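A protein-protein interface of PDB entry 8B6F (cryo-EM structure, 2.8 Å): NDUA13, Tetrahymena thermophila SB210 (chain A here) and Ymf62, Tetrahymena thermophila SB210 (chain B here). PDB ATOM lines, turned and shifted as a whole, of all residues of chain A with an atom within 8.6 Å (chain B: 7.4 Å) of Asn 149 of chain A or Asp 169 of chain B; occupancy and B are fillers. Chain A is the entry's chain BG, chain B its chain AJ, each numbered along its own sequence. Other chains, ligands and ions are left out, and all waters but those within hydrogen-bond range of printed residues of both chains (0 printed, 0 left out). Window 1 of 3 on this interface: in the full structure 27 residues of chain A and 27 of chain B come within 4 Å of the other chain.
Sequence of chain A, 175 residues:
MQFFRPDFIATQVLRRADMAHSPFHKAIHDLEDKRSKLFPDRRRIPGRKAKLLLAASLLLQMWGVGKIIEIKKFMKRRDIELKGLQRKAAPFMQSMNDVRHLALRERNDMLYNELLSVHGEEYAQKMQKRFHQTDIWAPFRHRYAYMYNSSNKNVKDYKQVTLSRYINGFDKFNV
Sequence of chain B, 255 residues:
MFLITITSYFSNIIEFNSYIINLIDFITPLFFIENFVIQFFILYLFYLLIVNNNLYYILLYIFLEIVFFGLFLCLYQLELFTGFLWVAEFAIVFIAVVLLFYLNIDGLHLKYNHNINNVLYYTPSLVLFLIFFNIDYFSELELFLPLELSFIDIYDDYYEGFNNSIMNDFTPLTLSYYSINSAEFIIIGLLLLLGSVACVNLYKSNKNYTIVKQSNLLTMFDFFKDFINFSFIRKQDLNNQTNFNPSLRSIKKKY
Printed residues of chain B within 4 Å of Met 147 of chain A: Glu 79 (3.3 Å), Leu 80 (3.4 Å) and Asp 169 (2.9 Å). Asn 149 of chain A touches three residues of chain B. Printed residues of chain A within 4 Å of Glu 79 of chain B: Met 147 (3.3 Å). Of the printed residues of chain A, Leu 80 of chain B touches Tyr 146 (3.96 Å) and Met 147 (3.4 Å). Of the printed residues of chain A, Ile 166 of chain B touches Asn 149. The nearest residue of chain A that does not touch Asp 169 of chain B is Ser 150 of chain A (5.4 Å).
The side-chain carboxylate (OE2) of Glu 160 of chain B lies within hydrogen-bond range of the side-chain amide nitrogen (ND2) of Asn 164 of chain B (3.3 Å). OD1 of Asn 164 of chain B is in hydrogen-bond range of N of Ile 166 of chain B, 2.7 Å away. The side-chain hydroxyl (OG) of Ser 151 of chain A is in hydrogen-bond range of the backbone carbonyl oxygen (O) of Tyr 148 of chain A (3.1 Å). OH of Tyr 148 of chain A sits at hydrogen-bond distance from NZ of Lys 153 of chain A, at 3.0 Å.
The side-chain amide oxygen (OD1) of Asn 149 of chain A lies within hydrogen-bond range of the side-chain amide nitrogen (ND2) of Asn 164 of chain B (3.0 Å). O of Ile 166 of chain B is in hydrogen-bond range of ND2 of Asn 149 of chain A (3.4 Å). The backbone carbonyl oxygen (O) of Asp 169 of chain B lies within hydrogen-bond range of the side-chain hydroxyl (OH) of Tyr 146 of chain A, 2.5 Å away. The side-chain carboxylate of Asp 169 of chain B sits at hydrogen-bond distance from the backbone NH of Tyr 148 of chain A (3.1 Å). The backbone NH (N) of Asn 149 of chain A sits at hydrogen-bond distance from the side-chain carboxylate (OD1) of Asp 169 of chain B (3.1 Å). The side-chain sulfur (SD) of Met 147 of chain A sits close to the side-chain carboxylate (OD2) of Asp 169 of chain B (3.4 Å).
Hydrophobic or aromatic side chains of chain B within 4 Å of the printed part of chain A: Leu 80, Phe 81, Ile 166 and Pro 172. Hydrophobic or aromatic side chains of chain A that line the printed part of chain B: Tyr 146 and Met 147.
Among the printed residues, merely in contact across the chains: Tyr 146 of chain A with Leu 80 of chain B, Tyr 146 of chain A with Phe 81 of chain B, Tyr 146 of chain A with Pro 172 of chain B, Met 147 of chain A with Glu 79 of chain B and Met 147 of chain A with Leu 80 of chain B.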
ATOM      1  N   ALA A 145      30.832 -17.028  -6.282  1.00  0.00           N
ATOM      2  CA  ALA A 145      29.916 -17.075  -5.154  1.00  0.00           C
ATOM      3  C   ALA A 145      29.052 -18.326  -5.218  1.00  0.00           C
ATOM      4  O   ALA A 145      28.586 -18.726  -6.289  1.00  0.00           O
ATOM      5  CB  ALA A 145      29.030 -15.831  -5.135  1.00  0.00           C
ATOM      6  N   TYR A 146      28.843 -18.950  -4.061  1.00  0.00           N
ATOM      7  CA  TYR A 146      28.002 -20.134  -3.948  1.00  0.00           C
ATOM      8  C   TYR A 146      26.794 -19.907  -3.054  1.00  0.00           C
ATOM      9  O   TYR A 146      25.661 -20.173  -3.472  1.00  0.00           O
ATOM     10  CB  TYR A 146      28.828 -21.314  -3.420  1.00  0.00           C
ATOM     11  CG  TYR A 146      27.992 -22.472  -2.931  1.00  0.00           C
ATOM     12  CD1 TYR A 146      27.367 -23.330  -3.824  1.00  0.00           C
ATOM     13  CD2 TYR A 146      27.839 -22.715  -1.575  1.00  0.00           C
ATOM     14  CE1 TYR A 146      26.606 -24.390  -3.377  1.00  0.00           C
ATOM     15  CE2 TYR A 146      27.080 -23.771  -1.120  1.00  0.00           C
ATOM     16  CZ  TYR A 146      26.468 -24.606  -2.025  1.00  0.00           C
ATOM     17  OH  TYR A 146      25.710 -25.662  -1.574  1.00  0.00           O
ATOM     18  N   MET A 147      27.001 -19.412  -1.838  1.00  0.00           N
ATOM     19  CA  MET A 147      25.914 -19.284  -0.882  1.00  0.00           C
ATOM     20  C   MET A 147      24.878 -18.275  -1.360  1.00  0.00           C
ATOM     21  O   MET A 147      25.183 -17.335  -2.099  1.00  0.00           O
ATOM     22  CB  MET A 147      26.455 -18.860   0.484  1.00  0.00           C
ATOM     23  CG  MET A 147      26.914 -20.006   1.372  1.00  0.00           C
ATOM     24  SD  MET A 147      25.536 -20.802   2.217  1.00  0.00           S
ATOM     25  CE  MET A 147      25.299 -22.253   1.200  1.00  0.00           C
ATOM     26  N   TYR A 148      23.638 -18.479  -0.919  1.00  0.00           N
ATOM     27  CA  TYR A 148      22.532 -17.570  -1.213  1.00  0.00           C
ATOM     28  C   TYR A 148      22.350 -17.390  -2.718  1.00  0.00           C
ATOM     29  O   TYR A 148      22.215 -16.277  -3.225  1.00  0.00           O
ATOM     30  CB  TYR A 148      22.738 -16.222  -0.520  1.00  0.00           C
ATOM     31  CG  TYR A 148      22.840 -16.339   0.980  1.00  0.00           C
ATOM     32  CD1 TYR A 148      21.705 -16.524   1.757  1.00  0.00           C
ATOM     33  CD2 TYR A 148      24.069 -16.270   1.618  1.00  0.00           C
ATOM     34  CE1 TYR A 148      21.792 -16.636   3.129  1.00  0.00           C
ATOM     35  CE2 TYR A 148      24.167 -16.379   2.989  1.00  0.00           C
ATOM     36  CZ  TYR A 148      23.024 -16.564   3.739  1.00  0.00           C
ATOM     37  OH  TYR A 148      23.115 -16.673   5.106  1.00  0.00           O
ATOM     38  N   ASN A 149      22.341 -18.512  -3.434  1.00  0.00           N
ATOM     39  CA  ASN A 149      22.125 -18.507  -4.877  1.00  0.00           C
ATOM     40  C   ASN A 149      23.159 -17.628  -5.578  1.00  0.00           C
ATOM     41  O   ASN A 149      22.833 -16.841  -6.468  1.00  0.00           O
ATOM     42  CB  ASN A 149      20.704 -18.049  -5.208  1.00  0.00           C
ATOM     43  CG  ASN A 149      20.276 -18.440  -6.603  1.00  0.00           C
ATOM     44  OD1 ASN A 149      21.094 -18.524  -7.517  1.00  0.00           O
ATOM     45  ND2 ASN A 149      18.983 -18.681  -6.777  1.00  0.00           N
ATOM     46  N   SER A 150      24.419 -17.760  -5.164  1.00  0.00           N
ATOM     47  CA  SER A 150      25.521 -16.972  -5.710  1.00  0.00           C
ATOM     48  C   SER A 150      25.269 -15.479  -5.504  1.00  0.00           C
ATOM     49  O   SER A 150      25.227 -14.686  -6.446  1.00  0.00           O
ATOM     50  CB  SER A 150      25.738 -17.295  -7.193  1.00  0.00           C
ATOM     51  OG  SER A 150      26.190 -18.628  -7.362  1.00  0.00           O
ATOM     52  N   SER A 151      25.094 -15.111  -4.238  1.00  0.00           N
ATOM     53  CA  SER A 151      24.893 -13.726  -3.845  1.00  0.00           C
ATOM     54  C   SER A 151      25.641 -13.478  -2.542  1.00  0.00           C
ATOM     55  O   SER A 151      26.233 -14.390  -1.960  1.00  0.00           O
ATOM     56  CB  SER A 151      23.405 -13.402  -3.701  1.00  0.00           C
ATOM     57  OG  SER A 151      22.699 -13.693  -4.894  1.00  0.00           O
ATOM     58  N   ASN A 152      25.615 -12.229  -2.087  1.00  0.00           N
ATOM     59  CA  ASN A 152      26.257 -11.825  -0.842  1.00  0.00           C
ATOM     60  C   ASN A 152      25.198 -11.275   0.102  1.00  0.00           C
ATOM     61  O   ASN A 152      24.563 -10.259  -0.200  1.00  0.00           O
ATOM     62  CB  ASN A 152      27.345 -10.782  -1.097  1.00  0.00           C
ATOM     63  CG  ASN A 152      28.530 -11.353  -1.843  1.00  0.00           C
ATOM     64  OD1 ASN A 152      29.456 -11.891  -1.238  1.00  0.00           O
ATOM     65  ND2 ASN A 152      28.505 -11.241  -3.165  1.00  0.00           N
ATOM     66  N   LYS A 153      25.010 -11.946   1.238  1.00  0.00           N
ATOM     67  CA  LYS A 153      24.035 -11.482   2.219  1.00  0.00           C
ATOM     68  C   LYS A 153      24.511 -10.209   2.907  1.00  0.00           C
ATOM     69  O   LYS A 153      23.749  -9.245   3.047  1.00  0.00           O
ATOM     70  CB  LYS A 153      23.769 -12.580   3.250  1.00  0.00           C
ATOM     71  CG  LYS A 153      22.778 -12.179   4.338  1.00  0.00           C
ATOM     72  CD  LYS A 153      22.539 -13.304   5.334  1.00  0.00           C
ATOM     73  CE  LYS A 153      23.775 -13.581   6.176  1.00  0.00           C
ATOM     74  NZ  LYS A 153      23.514 -14.609   7.223  1.00  0.00           N
ATOM     75  N   GLU B  79      29.033 -21.866   4.097  1.00  0.00           N
ATOM     76  CA  GLU B  79      28.367 -22.101   5.376  1.00  0.00           C
ATOM     77  C   GLU B  79      27.614 -23.425   5.392  1.00  0.00           C
ATOM     78  O   GLU B  79      27.638 -24.145   6.397  1.00  0.00           O
ATOM     79  CB  GLU B  79      27.413 -20.954   5.695  1.00  0.00           C
ATOM     80  CG  GLU B  79      28.092 -19.726   6.262  1.00  0.00           C
ATOM     81  CD  GLU B  79      28.974 -19.030   5.253  1.00  0.00           C
ATOM     82  OE1 GLU B  79      28.652 -19.077   4.050  1.00  0.00           O
ATOM     83  OE2 GLU B  79      29.990 -18.434   5.663  1.00  0.00           O
ATOM     84  N   LEU B  80      26.941 -23.764   4.294  1.00  0.00           N
ATOM     85  CA  LEU B  80      26.187 -25.012   4.252  1.00  0.00           C
ATOM     86  C   LEU B  80      27.105 -26.205   4.460  1.00  0.00           C
ATOM     87  O   LEU B  80      26.783 -27.120   5.227  1.00  0.00           O
ATOM     88  CB  LEU B  80      25.439 -25.125   2.925  1.00  0.00           C
ATOM     89  CG  LEU B  80      24.625 -26.397   2.675  1.00  0.00           C
ATOM     90  CD1 LEU B  80      23.384 -26.060   1.874  1.00  0.00           C
ATOM     91  CD2 LEU B  80      25.442 -27.455   1.950  1.00  0.00           C
ATOM     92  N   PHE B  81      28.258 -26.209   3.798  1.00  0.00           N
ATOM     93  CA  PHE B  81      29.204 -27.301   3.977  1.00  0.00           C
ATOM     94  C   PHE B  81      29.808 -27.289   5.375  1.00  0.00           C
ATOM     95  O   PHE B  81      30.120 -28.354   5.918  1.00  0.00           O
ATOM     96  CB  PHE B  81      30.284 -27.223   2.904  1.00  0.00           C
ATOM     97  CG  PHE B  81      29.749 -27.377   1.514  1.00  0.00           C
ATOM     98  CD1 PHE B  81      29.449 -28.632   1.012  1.00  0.00           C
ATOM     99  CD2 PHE B  81      29.526 -26.270   0.717  1.00  0.00           C
ATOM    100  CE1 PHE B  81      28.948 -28.780  -0.263  1.00  0.00           C
ATOM    101  CE2 PHE B  81      29.024 -26.411  -0.560  1.00  0.00           C
ATOM    102  CZ  PHE B  81      28.733 -27.668  -1.051  1.00  0.00           C
ATOM    103  N   PHE B  84      27.145 -29.024   7.487  1.00  0.00           N
ATOM    104  CA  PHE B  84      27.115 -30.455   7.208  1.00  0.00           C
ATOM    105  C   PHE B  84      28.336 -31.150   7.795  1.00  0.00           C
ATOM    106  O   PHE B  84      28.225 -32.242   8.363  1.00  0.00           O
ATOM    107  CB  PHE B  84      27.019 -30.700   5.706  1.00  0.00           C
ATOM    108  CG  PHE B  84      25.612 -30.693   5.198  1.00  0.00           C
ATOM    109  CD1 PHE B  84      24.785 -31.784   5.405  1.00  0.00           C
ATOM    110  CD2 PHE B  84      25.110 -29.592   4.530  1.00  0.00           C
ATOM    111  CE1 PHE B  84      23.485 -31.779   4.946  1.00  0.00           C
ATOM    112  CE2 PHE B  84      23.811 -29.580   4.069  1.00  0.00           C
ATOM    113  CZ  PHE B  84      22.996 -30.676   4.277  1.00  0.00           C
ATOM    114  N   GLU B 160      18.925 -12.720 -15.507  1.00  0.00           N
ATOM    115  CA  GLU B 160      19.094 -14.046 -14.927  1.00  0.00           C
ATOM    116  C   GLU B 160      18.485 -14.116 -13.535  1.00  0.00           C
ATOM    117  O   GLU B 160      17.978 -15.168 -13.131  1.00  0.00           O
ATOM    118  CB  GLU B 160      20.577 -14.417 -14.884  1.00  0.00           C
ATOM    119  CG  GLU B 160      20.850 -15.884 -14.573  1.00  0.00           C
ATOM    120  CD  GLU B 160      20.757 -16.212 -13.094  1.00  0.00           C
ATOM    121  OE1 GLU B 160      20.767 -15.273 -12.271  1.00  0.00           O
ATOM    122  OE2 GLU B 160      20.678 -17.411 -12.754  1.00  0.00           O
ATOM    123  N   GLY B 161      18.526 -13.013 -12.789  1.00  0.00           N
ATOM    124  CA  GLY B 161      17.942 -13.012 -11.458  1.00  0.00           C
ATOM    125  C   GLY B 161      16.447 -13.271 -11.471  1.00  0.00           C
ATOM    126  O   GLY B 161      15.941 -14.088 -10.700  1.00  0.00           O
ATOM    127  N   ASN B 164      15.627 -16.777 -12.469  1.00  0.00           N
ATOM    128  CA  ASN B 164      16.048 -17.794 -11.519  1.00  0.00           C
ATOM    129  C   ASN B 164      14.965 -17.993 -10.467  1.00  0.00           C
ATOM    130  O   ASN B 164      14.519 -17.029  -9.836  1.00  0.00           O
ATOM    131  CB  ASN B 164      17.365 -17.388 -10.858  1.00  0.00           C
ATOM    132  CG  ASN B 164      17.995 -18.515 -10.069  1.00  0.00           C
ATOM    133  OD1 ASN B 164      17.305 -19.410  -9.584  1.00  0.00           O
ATOM    134  ND2 ASN B 164      19.315 -18.477  -9.935  1.00  0.00           N
ATOM    135  N   SER B 165      14.548 -19.243 -10.278  1.00  0.00           N
ATOM    136  CA  SER B 165      13.518 -19.589  -9.309  1.00  0.00           C
ATOM    137  C   SER B 165      14.051 -20.392  -8.132  1.00  0.00           C
ATOM    138  O   SER B 165      13.262 -20.810  -7.278  1.00  0.00           O
ATOM    139  CB  SER B 165      12.391 -20.368  -9.998  1.00  0.00           C
ATOM    140  OG  SER B 165      12.879 -21.572 -10.565  1.00  0.00           O
ATOM    141  N   ILE B 166      15.362 -20.619  -8.060  1.00  0.00           N
ATOM    142  CA  ILE B 166      15.926 -21.422  -6.984  1.00  0.00           C
ATOM    143  C   ILE B 166      15.807 -20.678  -5.660  1.00  0.00           C
ATOM    144  O   ILE B 166      15.893 -19.444  -5.600  1.00  0.00           O
ATOM    145  CB  ILE B 166      17.392 -21.775  -7.300  1.00  0.00           C
ATOM    146  CG1 ILE B 166      17.467 -22.616  -8.577  1.00  0.00           C
ATOM    147  CG2 ILE B 166      18.034 -22.522  -6.137  1.00  0.00           C
ATOM    148  CD1 ILE B 166      18.855 -22.708  -9.164  1.00  0.00           C
ATOM    149  N   MET B 167      15.615 -21.440  -4.581  1.00  0.00           N
ATOM    150  CA  MET B 167      15.481 -20.877  -3.246  1.00  0.00           C
ATOM    151  C   MET B 167      16.350 -21.562  -2.200  1.00  0.00           C
ATOM    152  O   MET B 167      16.352 -21.125  -1.045  1.00  0.00           O
ATOM    153  CB  MET B 167      14.017 -20.936  -2.788  1.00  0.00           C
ATOM    154  CG  MET B 167      13.170 -19.797  -3.317  1.00  0.00           C
ATOM    155  SD  MET B 167      13.631 -18.204  -2.606  1.00  0.00           S
ATOM    156  CE  MET B 167      13.029 -18.390  -0.931  1.00  0.00           C
ATOM    157  N   ASN B 168      17.077 -22.617  -2.560  1.00  0.00           N
ATOM    158  CA  ASN B 168      17.964 -23.307  -1.638  1.00  0.00           C
ATOM    159  C   ASN B 168      19.337 -23.457  -2.279  1.00  0.00           C
ATOM    160  O   ASN B 168      19.498 -23.325  -3.494  1.00  0.00           O
ATOM    161  CB  ASN B 168      17.413 -24.683  -1.237  1.00  0.00           C
ATOM    162  CG  ASN B 168      17.200 -25.597  -2.425  1.00  0.00           C
ATOM    163  OD1 ASN B 168      18.117 -26.285  -2.868  1.00  0.00           O
ATOM    164  ND2 ASN B 168      15.979 -25.615  -2.945  1.00  0.00           N
ATOM    165  N   ASP B 169      20.332 -23.730  -1.436  1.00  0.00           N
ATOM    166  CA  ASP B 169      21.712 -23.883  -1.874  1.00  0.00           C
ATOM    167  C   ASP B 169      22.087 -25.339  -2.123  1.00  0.00           C
ATOM    168  O   ASP B 169      23.275 -25.674  -2.121  1.00  0.00           O
ATOM    169  CB  ASP B 169      22.660 -23.267  -0.845  1.00  0.00           C
ATOM    170  CG  ASP B 169      22.454 -21.777  -0.685  1.00  0.00           C
ATOM    171  OD1 ASP B 169      22.107 -21.115  -1.683  1.00  0.00           O
ATOM    172  OD2 ASP B 169      22.638 -21.268   0.440  1.00  0.00           O
ATOM    173  N   PHE B 170      21.102 -26.208  -2.329  1.00  0.00           N
ATOM    174  CA  PHE B 170      21.342 -27.610  -2.640  1.00  0.00           C
ATOM    175  C   PHE B 170      21.284 -27.896  -4.134  1.00  0.00           C
ATOM    176  O   PHE B 170      21.379 -29.060  -4.533  1.00  0.00           O
ATOM    177  CB  PHE B 170      20.332 -28.498  -1.910  1.00  0.00           C
ATOM    178  CG  PHE B 170      20.551 -28.578  -0.430  1.00  0.00           C
ATOM    179  CD1 PHE B 170      19.954 -27.667   0.424  1.00  0.00           C
ATOM    180  CD2 PHE B 170      21.344 -29.577   0.110  1.00  0.00           C
ATOM    181  CE1 PHE B 170      20.152 -27.744   1.788  1.00  0.00           C
ATOM    182  CE2 PHE B 170      21.546 -29.659   1.472  1.00  0.00           C
ATOM    183  CZ  PHE B 170      20.948 -28.744   2.313  1.00  0.00           C
ATOM    184  N   THR B 171      21.138 -26.868  -4.968  1.00  0.00           N
ATOM    185  CA  THR B 171      20.994 -27.101  -6.403  1.00  0.00           C
ATOM    186  C   THR B 171      22.220 -27.769  -7.006  1.00  0.00           C
ATOM    187  O   THR B 171      22.057 -28.751  -7.750  1.00  0.00           O
ATOM    188  CB  THR B 171      20.662 -25.784  -7.112  1.00  0.00           C
ATOM    189  OG1 THR B 171      19.365 -25.336  -6.702  1.00  0.00           O
ATOM    190  CG2 THR B 171      20.669 -25.964  -8.627  1.00  0.00           C
ATOM    191  N   PRO B 172      23.448 -27.304  -6.766  1.00  0.00           N
ATOM    192  CA  PRO B 172      24.601 -28.058  -7.282  1.00  0.00           C
ATOM    193  C   PRO B 172      24.668 -29.473  -6.744  1.00  0.00           C
ATOM    194  O   PRO B 172      25.048 -30.396  -7.473  1.00  0.00           O
ATOM    195  CB  PRO B 172      25.803 -27.216  -6.829  1.00  0.00           C
ATOM    196  CG  PRO B 172      25.253 -25.867  -6.566  1.00  0.00           C
ATOM    197  CD  PRO B 172      23.871 -26.089  -6.050  1.00  0.00           C
ATOM    198  N   LEU B 173      24.314 -29.669  -5.474  1.00  0.00           N
ATOM    199  CA  LEU B 173      24.384 -31.002  -4.888  1.00  0.00           C
ATOM    200  C   LEU B 173      23.413 -31.959  -5.569  1.00  0.00           C
ATOM    201  O   LEU B 173      23.760 -33.113  -5.843  1.00  0.00           O
ATOM    202  CB  LEU B 173      24.108 -30.918  -3.387  1.00  0.00           C
ATOM    203  CG  LEU B 173      25.140 -30.120  -2.582  1.00  0.00           C
ATOM    204  CD1 LEU B 173      24.707 -29.992  -1.133  1.00  0.00           C
ATOM    205  CD2 LEU B 173      26.521 -30.752  -2.667  1.00  0.00           C
ATOM    206  N   THR B 174      22.189 -31.503  -5.846  1.00  0.00           N
ATOM    207  CA  THR B 174      21.228 -32.363  -6.533  1.00  0.00           C
ATOM    208  C   THR B 174      21.625 -32.586  -7.986  1.00  0.00           C
ATOM    209  O   THR B 174      21.503 -33.703  -8.504  1.00  0.00           O
ATOM    210  CB  THR B 174      19.816 -31.779  -6.439  1.00  0.00           C
ATOM    211  OG1 THR B 174      18.894 -32.640  -7.122  1.00  0.00           O
ATOM    212  CG2 THR B 174      19.744 -30.399  -7.051  1.00  0.00           C
